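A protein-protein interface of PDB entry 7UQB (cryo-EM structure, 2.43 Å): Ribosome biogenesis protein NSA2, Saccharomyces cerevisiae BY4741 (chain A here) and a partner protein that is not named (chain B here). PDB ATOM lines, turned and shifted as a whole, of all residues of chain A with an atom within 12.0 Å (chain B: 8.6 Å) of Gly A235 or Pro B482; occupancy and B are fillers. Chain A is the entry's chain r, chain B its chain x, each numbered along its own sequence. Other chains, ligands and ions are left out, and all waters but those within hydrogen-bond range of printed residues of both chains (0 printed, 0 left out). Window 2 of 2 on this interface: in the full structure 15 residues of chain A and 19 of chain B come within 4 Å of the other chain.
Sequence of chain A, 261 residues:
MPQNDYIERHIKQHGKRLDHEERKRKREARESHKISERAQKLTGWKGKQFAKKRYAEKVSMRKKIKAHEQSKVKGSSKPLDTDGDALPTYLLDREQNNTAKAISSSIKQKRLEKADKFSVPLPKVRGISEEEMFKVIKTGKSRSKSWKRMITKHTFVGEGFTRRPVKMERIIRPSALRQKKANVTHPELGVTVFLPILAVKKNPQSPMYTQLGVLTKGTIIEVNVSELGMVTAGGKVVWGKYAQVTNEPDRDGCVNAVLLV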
ATOM      1  N   SER A 226      -1.007  -4.484   2.945  1.00  0.00           N
ATOM      2  CA  SER A 226      -2.028  -5.416   2.473  1.00  0.00           C
ATOM      3  C   SER A 226      -2.355  -6.473   3.521  1.00  0.00           C
ATOM      4  O   SER A 226      -3.516  -6.868   3.674  1.00  0.00           O
ATOM      5  CB  SER A 226      -1.569  -6.085   1.179  1.00  0.00           C
ATOM      6  OG  SER A 226      -1.063  -5.139   0.258  1.00  0.00           O
ATOM      7  N   GLY A 229      -4.998  -5.860   6.596  1.00  0.00           N
ATOM      8  CA  GLY A 229      -6.435  -5.967   6.401  1.00  0.00           C
ATOM      9  C   GLY A 229      -7.232  -4.706   6.662  1.00  0.00           C
ATOM     10  O   GLY A 229      -8.331  -4.782   7.225  1.00  0.00           O
ATOM     11  N   MET A 230      -6.713  -3.550   6.263  1.00  0.00           N
ATOM     12  CA  MET A 230      -7.393  -2.280   6.478  1.00  0.00           C
ATOM     13  C   MET A 230      -8.354  -2.008   5.327  1.00  0.00           C
ATOM     14  O   MET A 230      -8.013  -2.221   4.160  1.00  0.00           O
ATOM     15  CB  MET A 230      -6.378  -1.146   6.609  1.00  0.00           C
ATOM     16  CG  MET A 230      -5.156  -1.522   7.431  1.00  0.00           C
ATOM     17  SD  MET A 230      -3.959  -0.187   7.591  1.00  0.00           S
ATOM     18  CE  MET A 230      -4.859   0.943   8.646  1.00  0.00           C
ATOM     19  N   VAL A 231      -9.559  -1.548   5.663  1.00  0.00           N
ATOM     20  CA  VAL A 231     -10.610  -1.254   4.695  1.00  0.00           C
ATOM     21  C   VAL A 231     -11.164   0.131   5.003  1.00  0.00           C
ATOM     22  O   VAL A 231     -11.413   0.457   6.168  1.00  0.00           O
ATOM     23  CB  VAL A 231     -11.732  -2.313   4.733  1.00  0.00           C
ATOM     24  CG1 VAL A 231     -12.890  -1.915   3.836  1.00  0.00           C
ATOM     25  CG2 VAL A 231     -11.203  -3.675   4.323  1.00  0.00           C
ATOM     26  N   THR A 232     -11.351   0.943   3.964  1.00  0.00           N
ATOM     27  CA  THR A 232     -11.899   2.279   4.140  1.00  0.00           C
ATOM     28  C   THR A 232     -13.375   2.214   4.527  1.00  0.00           C
ATOM     29  O   THR A 232     -14.019   1.163   4.475  1.00  0.00           O
ATOM     30  CB  THR A 232     -11.751   3.106   2.862  1.00  0.00           C
ATOM     31  OG1 THR A 232     -12.613   2.579   1.847  1.00  0.00           O
ATOM     32  CG2 THR A 232     -10.322   3.085   2.364  1.00  0.00           C
ATOM     33  N   ALA A 233     -13.914   3.371   4.918  1.00  0.00           N
ATOM     34  CA  ALA A 233     -15.343   3.466   5.192  1.00  0.00           C
ATOM     35  C   ALA A 233     -16.169   3.273   3.927  1.00  0.00           C
ATOM     36  O   ALA A 233     -17.334   2.869   4.005  1.00  0.00           O
ATOM     37  CB  ALA A 233     -15.668   4.810   5.841  1.00  0.00           C
ATOM     38  N   GLY A 234     -15.588   3.553   2.763  1.00  0.00           N
ATOM     39  CA  GLY A 234     -16.214   3.310   1.483  1.00  0.00           C
ATOM     40  C   GLY A 234     -16.023   1.922   0.919  1.00  0.00           C
ATOM     41  O   GLY A 234     -16.540   1.627  -0.163  1.00  0.00           O
ATOM     42  N   GLY A 235     -15.290   1.052   1.613  1.00  0.00           N
ATOM     43  CA  GLY A 235     -15.131  -0.328   1.213  1.00  0.00           C
ATOM     44  C   GLY A 235     -13.834  -0.660   0.503  1.00  0.00           C
ATOM     45  O   GLY A 235     -13.578  -1.844   0.251  1.00  0.00           O
ATOM     46  N   LYS A 236     -13.015   0.332   0.172  1.00  0.00           N
ATOM     47  CA  LYS A 236     -11.772   0.074  -0.541  1.00  0.00           C
ATOM     48  C   LYS A 236     -10.720  -0.526   0.384  1.00  0.00           C
ATOM     49  O   LYS A 236     -10.593  -0.133   1.547  1.00  0.00           O
ATOM     50  CB  LYS A 236     -11.235   1.360  -1.170  1.00  0.00           C
ATOM     51  CG  LYS A 236     -11.573   1.528  -2.639  1.00  0.00           C
ATOM     52  CD  LYS A 236     -12.962   2.098  -2.839  1.00  0.00           C
ATOM     53  CE  LYS A 236     -13.214   2.406  -4.306  1.00  0.00           C
ATOM     54  NZ  LYS A 236     -14.495   3.135  -4.507  1.00  0.00           N
ATOM     55  N   VAL A 237      -9.961  -1.477  -0.147  1.00  0.00           N
ATOM     56  CA  VAL A 237      -8.883  -2.114   0.600  1.00  0.00           C
ATOM     57  C   VAL A 237      -7.659  -1.212   0.570  1.00  0.00           C
ATOM     58  O   VAL A 237      -7.199  -0.806  -0.502  1.00  0.00           O
ATOM     59  CB  VAL A 237      -8.563  -3.500   0.019  1.00  0.00           C
ATOM     60  CG1 VAL A 237      -7.453  -4.169   0.816  1.00  0.00           C
ATOM     61  CG2 VAL A 237      -9.810  -4.366  -0.010  1.00  0.00           C
ATOM     62  N   VAL A 238      -7.124  -0.900   1.746  1.00  0.00           N
ATOM     63  CA  VAL A 238      -5.924  -0.079   1.866  1.00  0.00           C
ATOM     64  C   VAL A 238      -4.706  -0.987   1.778  1.00  0.00           C
ATOM     65  O   VAL A 238      -4.547  -1.909   2.585  1.00  0.00           O
ATOM     66  CB  VAL A 238      -5.921   0.713   3.181  1.00  0.00           C
ATOM     67  CG1 VAL A 238      -4.611   1.466   3.341  1.00  0.00           C
ATOM     68  CG2 VAL A 238      -7.092   1.664   3.229  1.00  0.00           C
ATOM     69  N   TRP A 239      -3.840  -0.727   0.798  1.00  0.00           N
ATOM     70  CA  TRP A 239      -2.594  -1.471   0.671  1.00  0.00           C
ATOM     71  C   TRP A 239      -1.378  -0.557   0.599  1.00  0.00           C
ATOM     72  O   TRP A 239      -0.276  -1.036   0.317  1.00  0.00           O
ATOM     73  CB  TRP A 239      -2.629  -2.400  -0.549  1.00  0.00           C
ATOM     74  CG  TRP A 239      -2.579  -1.712  -1.877  1.00  0.00           C
ATOM     75  CD1 TRP A 239      -3.612  -1.100  -2.522  1.00  0.00           C
ATOM     76  CD2 TRP A 239      -1.439  -1.588  -2.738  1.00  0.00           C
ATOM     77  NE1 TRP A 239      -3.185  -0.592  -3.721  1.00  0.00           N
ATOM     78  CE2 TRP A 239      -1.856  -0.879  -3.880  1.00  0.00           C
ATOM     79  CE3 TRP A 239      -0.107  -2.005  -2.653  1.00  0.00           C
ATOM     80  CZ2 TRP A 239      -0.987  -0.576  -4.928  1.00  0.00           C
ATOM     81  CZ3 TRP A 239       0.752  -1.700  -3.691  1.00  0.00           C
ATOM     82  CH2 TRP A 239       0.308  -0.995  -4.814  1.00  0.00           C
ATOM     83  N   THR B 132     -28.463  -5.452   0.172  1.00  0.00           N
ATOM     84  CA  THR B 132     -27.604  -4.531  -0.556  1.00  0.00           C
ATOM     85  C   THR B 132     -27.311  -3.237   0.184  1.00  0.00           C
ATOM     86  O   THR B 132     -26.461  -2.468  -0.276  1.00  0.00           O
ATOM     87  CB  THR B 132     -28.224  -4.184  -1.918  1.00  0.00           C
ATOM     88  OG1 THR B 132     -29.629  -3.952  -1.758  1.00  0.00           O
ATOM     89  CG2 THR B 132     -28.007  -5.313  -2.910  1.00  0.00           C
ATOM     90  N   ARG B 133     -27.976  -2.969   1.302  1.00  0.00           N
ATOM     91  CA  ARG B 133     -27.798  -1.713   2.008  1.00  0.00           C
ATOM     92  C   ARG B 133     -28.142  -1.924   3.472  1.00  0.00           C
ATOM     93  O   ARG B 133     -28.864  -2.856   3.831  1.00  0.00           O
ATOM     94  CB  ARG B 133     -28.671  -0.611   1.403  1.00  0.00           C
ATOM     95  CG  ARG B 133     -30.144  -0.968   1.371  1.00  0.00           C
ATOM     96  CD  ARG B 133     -30.948   0.041   0.578  1.00  0.00           C
ATOM     97  NE  ARG B 133     -32.380  -0.159   0.758  1.00  0.00           N
ATOM     98  CZ  ARG B 133     -33.086   0.365   1.751  1.00  0.00           C
ATOM     99  NH1 ARG B 133     -32.521   1.130   2.670  1.00  0.00           N
ATOM    100  NH2 ARG B 133     -34.388   0.113   1.824  1.00  0.00           N
ATOM    101  N   SER B 134     -27.624  -1.040   4.315  1.00  0.00           N
ATOM    102  CA  SER B 134     -27.908  -1.106   5.739  1.00  0.00           C
ATOM    103  C   SER B 134     -29.264  -0.473   6.006  1.00  0.00           C
ATOM    104  O   SER B 134     -29.462   0.716   5.737  1.00  0.00           O
ATOM    105  CB  SER B 134     -26.818  -0.402   6.543  1.00  0.00           C
ATOM    106  OG  SER B 134     -27.039  -0.564   7.934  1.00  0.00           O
ATOM    107  N   GLY B 441     -11.964 -12.570  -1.196  1.00  0.00           N
ATOM    108  CA  GLY B 441     -12.367 -11.180  -1.171  1.00  0.00           C
ATOM    109  C   GLY B 441     -12.247 -10.542   0.195  1.00  0.00           C
ATOM    110  O   GLY B 441     -12.052  -9.328   0.298  1.00  0.00           O
ATOM    111  N   VAL B 443     -10.105  -9.623   3.392  1.00  0.00           N
ATOM    112  CA  VAL B 443      -8.690  -9.347   3.604  1.00  0.00           C
ATOM    113  C   VAL B 443      -8.263  -9.584   5.039  1.00  0.00           C
ATOM    114  O   VAL B 443      -7.092  -9.359   5.372  1.00  0.00           O
ATOM    115  CB  VAL B 443      -8.326  -7.918   3.160  1.00  0.00           C
ATOM    116  CG1 VAL B 443      -8.574  -7.758   1.671  1.00  0.00           C
ATOM    117  CG2 VAL B 443      -9.124  -6.899   3.950  1.00  0.00           C
ATOM    118  N   ASP B 464     -12.186  -7.810   8.959  1.00  0.00           N
ATOM    119  CA  ASP B 464     -11.918  -6.605   8.178  1.00  0.00           C
ATOM    120  C   ASP B 464     -13.073  -5.607   8.202  1.00  0.00           C
ATOM    121  O   ASP B 464     -13.151  -4.758   7.305  1.00  0.00           O
ATOM    122  CB  ASP B 464     -11.555  -6.972   6.731  1.00  0.00           C
ATOM    123  CG  ASP B 464     -12.647  -7.761   6.004  1.00  0.00           C
ATOM    124  OD1 ASP B 464     -13.846  -7.617   6.313  1.00  0.00           O
ATOM    125  OD2 ASP B 464     -12.292  -8.537   5.095  1.00  0.00           O
ATOM    126  N   THR B 465     -13.962  -5.718   9.194  1.00  0.00           N
ATOM    127  CA  THR B 465     -15.090  -4.816   9.443  1.00  0.00           C
ATOM    128  C   THR B 465     -16.138  -4.850   8.335  1.00  0.00           C
ATOM    129  O   THR B 465     -16.946  -3.925   8.221  1.00  0.00           O
ATOM    130  CB  THR B 465     -14.632  -3.364   9.668  1.00  0.00           C
ATOM    131  OG1 THR B 465     -14.287  -2.769   8.411  1.00  0.00           O
ATOM    132  CG2 THR B 465     -13.424  -3.296  10.602  1.00  0.00           C
ATOM    133  N   THR B 466     -16.168  -5.897   7.511  1.00  0.00           N
ATOM    134  CA  THR B 466     -17.104  -5.952   6.397  1.00  0.00           C
ATOM    135  C   THR B 466     -17.911  -7.241   6.414  1.00  0.00           C
ATOM    136  O   THR B 466     -17.456  -8.291   6.893  1.00  0.00           O
ATOM    137  CB  THR B 466     -16.397  -5.830   5.029  1.00  0.00           C
ATOM    138  OG1 THR B 466     -15.470  -6.909   4.863  1.00  0.00           O
ATOM    139  CG2 THR B 466     -15.664  -4.501   4.908  1.00  0.00           C
ATOM    140  N   LEU B 467     -19.128  -7.136   5.883  1.00  0.00           N
ATOM    141  CA  LEU B 467     -19.929  -8.283   5.495  1.00  0.00           C
ATOM    142  C   LEU B 467     -19.796  -8.490   3.994  1.00  0.00           C
ATOM    143  O   LEU B 467     -19.543  -7.551   3.239  1.00  0.00           O
ATOM    144  CB  LEU B 467     -21.403  -8.089   5.858  1.00  0.00           C
ATOM    145  CG  LEU B 467     -21.913  -8.579   7.212  1.00  0.00           C
ATOM    146  CD1 LEU B 467     -21.229  -7.853   8.354  1.00  0.00           C
ATOM    147  CD2 LEU B 467     -23.419  -8.400   7.288  1.00  0.00           C
ATOM    148  N   LYS B 468     -19.957  -9.733   3.565  1.00  0.00           N
ATOM    149  CA  LYS B 468     -19.931 -10.038   2.143  1.00  0.00           C
ATOM    150  C   LYS B 468     -21.016 -11.051   1.828  1.00  0.00           C
ATOM    151  O   LYS B 468     -21.154 -12.056   2.530  1.00  0.00           O
ATOM    152  CB  LYS B 468     -18.556 -10.555   1.706  1.00  0.00           C
ATOM    153  CG  LYS B 468     -17.544  -9.443   1.492  1.00  0.00           C
ATOM    154  CD  LYS B 468     -16.184  -9.969   1.088  1.00  0.00           C
ATOM    155  CE  LYS B 468     -15.291  -8.835   0.619  1.00  0.00           C
ATOM    156  NZ  LYS B 468     -15.225  -7.723   1.601  1.00  0.00           N
ATOM    157  N   VAL B 479     -22.146  -8.974  -3.347  1.00  0.00           N
ATOM    158  CA  VAL B 479     -22.083  -7.586  -2.896  1.00  0.00           C
ATOM    159  C   VAL B 479     -21.233  -7.503  -1.633  1.00  0.00           C
ATOM    160  O   VAL B 479     -21.231  -8.415  -0.804  1.00  0.00           O
ATOM    161  CB  VAL B 479     -23.508  -7.003  -2.696  1.00  0.00           C
ATOM    162  CG1 VAL B 479     -24.269  -7.758  -1.635  1.00  0.00           C
ATOM    163  CG2 VAL B 479     -23.465  -5.513  -2.386  1.00  0.00           C
ATOM    164  N   ASP B 480     -20.489  -6.408  -1.506  1.00  0.00           N
ATOM    165  CA  ASP B 480     -19.622  -6.147  -0.364  1.00  0.00           C
ATOM    166  C   ASP B 480     -20.234  -5.023   0.463  1.00  0.00           C
ATOM    167  O   ASP B 480     -20.466  -3.926  -0.055  1.00  0.00           O
ATOM    168  CB  ASP B 480     -18.217  -5.773  -0.834  1.00  0.00           C
ATOM    169  CG  ASP B 480     -17.253  -5.553   0.313  1.00  0.00           C
ATOM    170  OD1 ASP B 480     -17.484  -6.106   1.408  1.00  0.00           O
ATOM    171  OD2 ASP B 480     -16.262  -4.819   0.118  1.00  0.00           O
ATOM    172  N   LEU B 481     -20.490  -5.293   1.744  1.00  0.00           N
ATOM    173  CA  LEU B 481     -21.194  -4.364   2.621  1.00  0.00           C
ATOM    174  C   LEU B 481     -20.256  -3.851   3.706  1.00  0.00           C
ATOM    175  O   LEU B 481     -19.968  -4.575   4.675  1.00  0.00           O
ATOM    176  CB  LEU B 481     -22.410  -5.051   3.248  1.00  0.00           C
ATOM    177  CG  LEU B 481     -23.362  -5.766   2.286  1.00  0.00           C
ATOM    178  CD1 LEU B 481     -24.415  -6.548   3.046  1.00  0.00           C
ATOM    179  CD2 LEU B 481     -24.013  -4.770   1.345  1.00  0.00           C
ATOM    180  N   PRO B 482     -19.720  -2.635   3.575  1.00  0.00           N
ATOM    181  CA  PRO B 482     -19.035  -2.004   4.707  1.00  0.00           C
ATOM    182  C   PRO B 482     -20.001  -1.184   5.548  1.00  0.00           C
ATOM    183  O   PRO B 482     -21.187  -1.094   5.224  1.00  0.00           O
ATOM    184  CB  PRO B 482     -17.984  -1.123   4.024  1.00  0.00           C
ATOM    185  CG  PRO B 482     -18.640  -0.728   2.746  1.00  0.00           C
ATOM    186  CD  PRO B 482     -19.489  -1.904   2.316  1.00  0.00           C
ATOM    187  N   GLY B 483     -19.507  -0.575   6.620  1.00  0.00           N
ATOM    188  CA  GLY B 483     -20.356   0.231   7.475  1.00  0.00           C
ATOM    189  C   GLY B 483     -20.044   0.079   8.947  1.00  0.00           C
ATOM    190  O   GLY B 483     -20.197   1.031   9.718  1.00  0.00           O
ATOM    191  N   HIS B 484     -19.600  -1.106   9.350  1.00  0.00           N
ATOM    192  CA  HIS B 484     -19.132  -1.293  10.715  1.00  0.00           C
ATOM    193  C   HIS B 484     -17.810  -0.567  10.910  1.00  0.00           C
ATOM    194  O   HIS B 484     -16.950  -0.560  10.026  1.00  0.00           O
ATOM    195  CB  HIS B 484     -18.965  -2.778  11.031  1.00  0.00           C
ATOM    196  CG  HIS B 484     -20.247  -3.487  11.328  1.00  0.00           C
ATOM    197  ND1 HIS B 484     -20.792  -3.539  12.591  1.00  0.00           N
ATOM    198  CD2 HIS B 484     -21.082  -4.191  10.528  1.00  0.00           C
ATOM    199  CE1 HIS B 484     -21.911  -4.240  12.559  1.00  0.00           C
ATOM    200  NE2 HIS B 484     -22.111  -4.645  11.318  1.00  0.00           N
ATOM    201  N   LYS B 485     -17.653   0.053  12.077  1.00  0.00           N
ATOM    202  CA  LYS B 485     -16.435   0.784  12.396  1.00  0.00           C
ATOM    203  C   LYS B 485     -15.352  -0.095  13.004  1.00  0.00           C
ATOM    204  O   LYS B 485     -14.226   0.377  13.189  1.00  0.00           O
ATOM    205  CB  LYS B 485     -16.748   1.937  13.355  1.00  0.00           C
ATOM    206  CG  LYS B 485     -17.881   2.844  12.899  1.00  0.00           C
ATOM    207  CD  LYS B 485     -17.612   3.414  11.517  1.00  0.00           C
ATOM    208  CE  LYS B 485     -18.730   4.343  11.072  1.00  0.00           C
ATOM    209  NZ  LYS B 485     -18.827   5.553  11.935  1.00  0.00           N
ATOM    210  N   VAL B 488     -16.476  -7.226  13.094  1.00  0.00           N
ATOM    211  CA  VAL B 488     -17.816  -7.787  13.209  1.00  0.00           C
ATOM    212  C   VAL B 488     -17.694  -9.201  13.754  1.00  0.00           C
ATOM    213  O   VAL B 488     -16.941 -10.022  13.217  1.00  0.00           O
ATOM    214  CB  VAL B 488     -18.542  -7.774  11.855  1.00  0.00           C
ATOM    215  CG1 VAL B 488     -20.017  -8.086  12.047  1.00  0.00           C
ATOM    216  CG2 VAL B 488     -18.359  -6.433  11.171  1.00  0.00           C
ATOM    217  N   SER B 502     -26.069  -7.818  11.953  1.00  0.00           N
ATOM    218  CA  SER B 502     -24.641  -7.931  12.199  1.00  0.00           C
ATOM    219  C   SER B 502     -24.259  -7.096  13.412  1.00  0.00           C
ATOM    220  O   SER B 502     -24.828  -6.028  13.663  1.00  0.00           O
ATOM    221  CB  SER B 502     -23.821  -7.502  10.976  1.00  0.00           C
ATOM    222  OG  SER B 502     -24.004  -6.130  10.684  1.00  0.00           O
ATOM    223  N   ARG B 510     -26.259  -3.494  13.218  1.00  0.00           N
ATOM    224  CA  ARG B 510     -26.554  -3.121  11.843  1.00  0.00           C
ATOM    225  C   ARG B 510     -27.605  -4.075  11.296  1.00  0.00           C
ATOM    226  O   ARG B 510     -27.418  -5.296  11.321  1.00  0.00           O
ATOM    227  CB  ARG B 510     -25.300  -3.152  10.970  1.00  0.00           C
ATOM    228  CG  ARG B 510     -24.249  -2.132  11.357  1.00  0.00           C
ATOM    229  CD  ARG B 510     -24.800  -0.737  11.325  1.00  0.00           C
ATOM    230  NE  ARG B 510     -24.787  -0.153   9.990  1.00  0.00           N
ATOM    231  CZ  ARG B 510     -23.961   0.811   9.606  1.00  0.00           C
ATOM    232  NH1 ARG B 510     -23.065   1.324  10.433  1.00  0.00           N
ATOM    233  NH2 ARG B 510     -24.041   1.275   8.363  1.00  0.00           N
ATOM    234  N   TRP B 512     -29.562  -4.965   7.770  1.00  0.00           N
ATOM    235  CA  TRP B 512     -29.401  -4.868   6.327  1.00  0.00           C
ATOM    236  C   TRP B 512     -30.593  -5.520   5.646  1.00  0.00           C
ATOM    237  O   TRP B 512     -31.120  -6.526   6.130  1.00  0.00           O
ATOM    238  CB  TRP B 512     -28.122  -5.569   5.847  1.00  0.00           C
ATOM    239  CG  TRP B 512     -26.913  -5.351   6.700  1.00  0.00           C
ATOM    240  CD1 TRP B 512     -26.636  -5.943   7.898  1.00  0.00           C
ATOM    241  CD2 TRP B 512     -25.801  -4.503   6.406  1.00  0.00           C
ATOM    242  NE1 TRP B 512     -25.430  -5.501   8.375  1.00  0.00           N
ATOM    243  CE2 TRP B 512     -24.894  -4.619   7.476  1.00  0.00           C
ATOM    244  CE3 TRP B 512     -25.485  -3.654   5.343  1.00  0.00           C
ATOM    245  CZ2 TRP B 512     -23.696  -3.915   7.514  1.00  0.00           C
ATOM    246  CZ3 TRP B 512     -24.297  -2.953   5.386  1.00  0.00           C
ATOM    247  CH2 TRP B 512     -23.417  -3.089   6.462  1.00  0.00           C
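N of Gly A235 is in hydrogen-bond range of OG1 of Thr A232 (3.1 Å). The backbone NH of Val B443 is in hydrogen-bond range of the side-chain carboxylate of Asp B464. OD1 of Asp B464 sits at hydrogen-bond distance from N of Thr B466 (3.1 Å). The side-chain hydroxyl (OG1) of Thr B466 sits at hydrogen-bond distance from the side-chain amino group (NZ) of Lys B468.
Val B443 touches Gly A229. CB of Asp B464 touches O of Gly A229, 3.9 Å away. CG2 of Val A231 touches CG2 of Val B443 (3.9 Å). O of Asp B464 touches CG2 of Val A231 (3.7 Å). Thr B466 touches Val A231. CG of Pro B482 touches CA of Gly A235 (3.9 Å). Val B443 touches Val A237.
Of the printed residues of chain B, Gly A229 touches Val B443 and Asp B464. Printed residues of chain B within 4 Å of Val A231: Val B443 (3.9 Å), Asp B464 (3.7 Å) and Thr B466 (3.9 Å). Of the printed residues of chain B, Gly A235 touches Pro B482. Of the printed residues of chain B, Val A237 touches Val B443 (3.9 Å). Printed residues of chain A within 4 Å of Val B443: Gly A229 (3.6 Å), Val A231 (3.9 Å) and Val A237 (3.9 Å). No residue of chain A comes within 4 Å of Leu B467. No residue of chain A comes within 4 Å of Leu B481. Pro B482 touches just one residue of chain A: Gly A235 (3.9 Å). No residue of chain A comes within 4 Å of Gly B483. No residue of chain A comes within 4 Å of His B484. The nearest residue of chain A that does not touch Pro B482 is Ala A233 (4.03 Å). The nearest printed residue of chain B that does not touch Val A231 is Thr B465 (4.5 Å).
Of the 12 printed residues of chain A, 4 touch a printed residue of chain B. Of the 21 printed residues of chain B, 4 touch a printed residue of chain A. Printed residues of chain B that touch a printed residue of chain A: Val B443, Asp B464, Thr B466 and Pro B482. Hydrophobic or aromatic side chains of chain B that line the printed part of chain A: Val B443 and Pro B482. Among the printed residues, 7 pairs touch across the chains.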
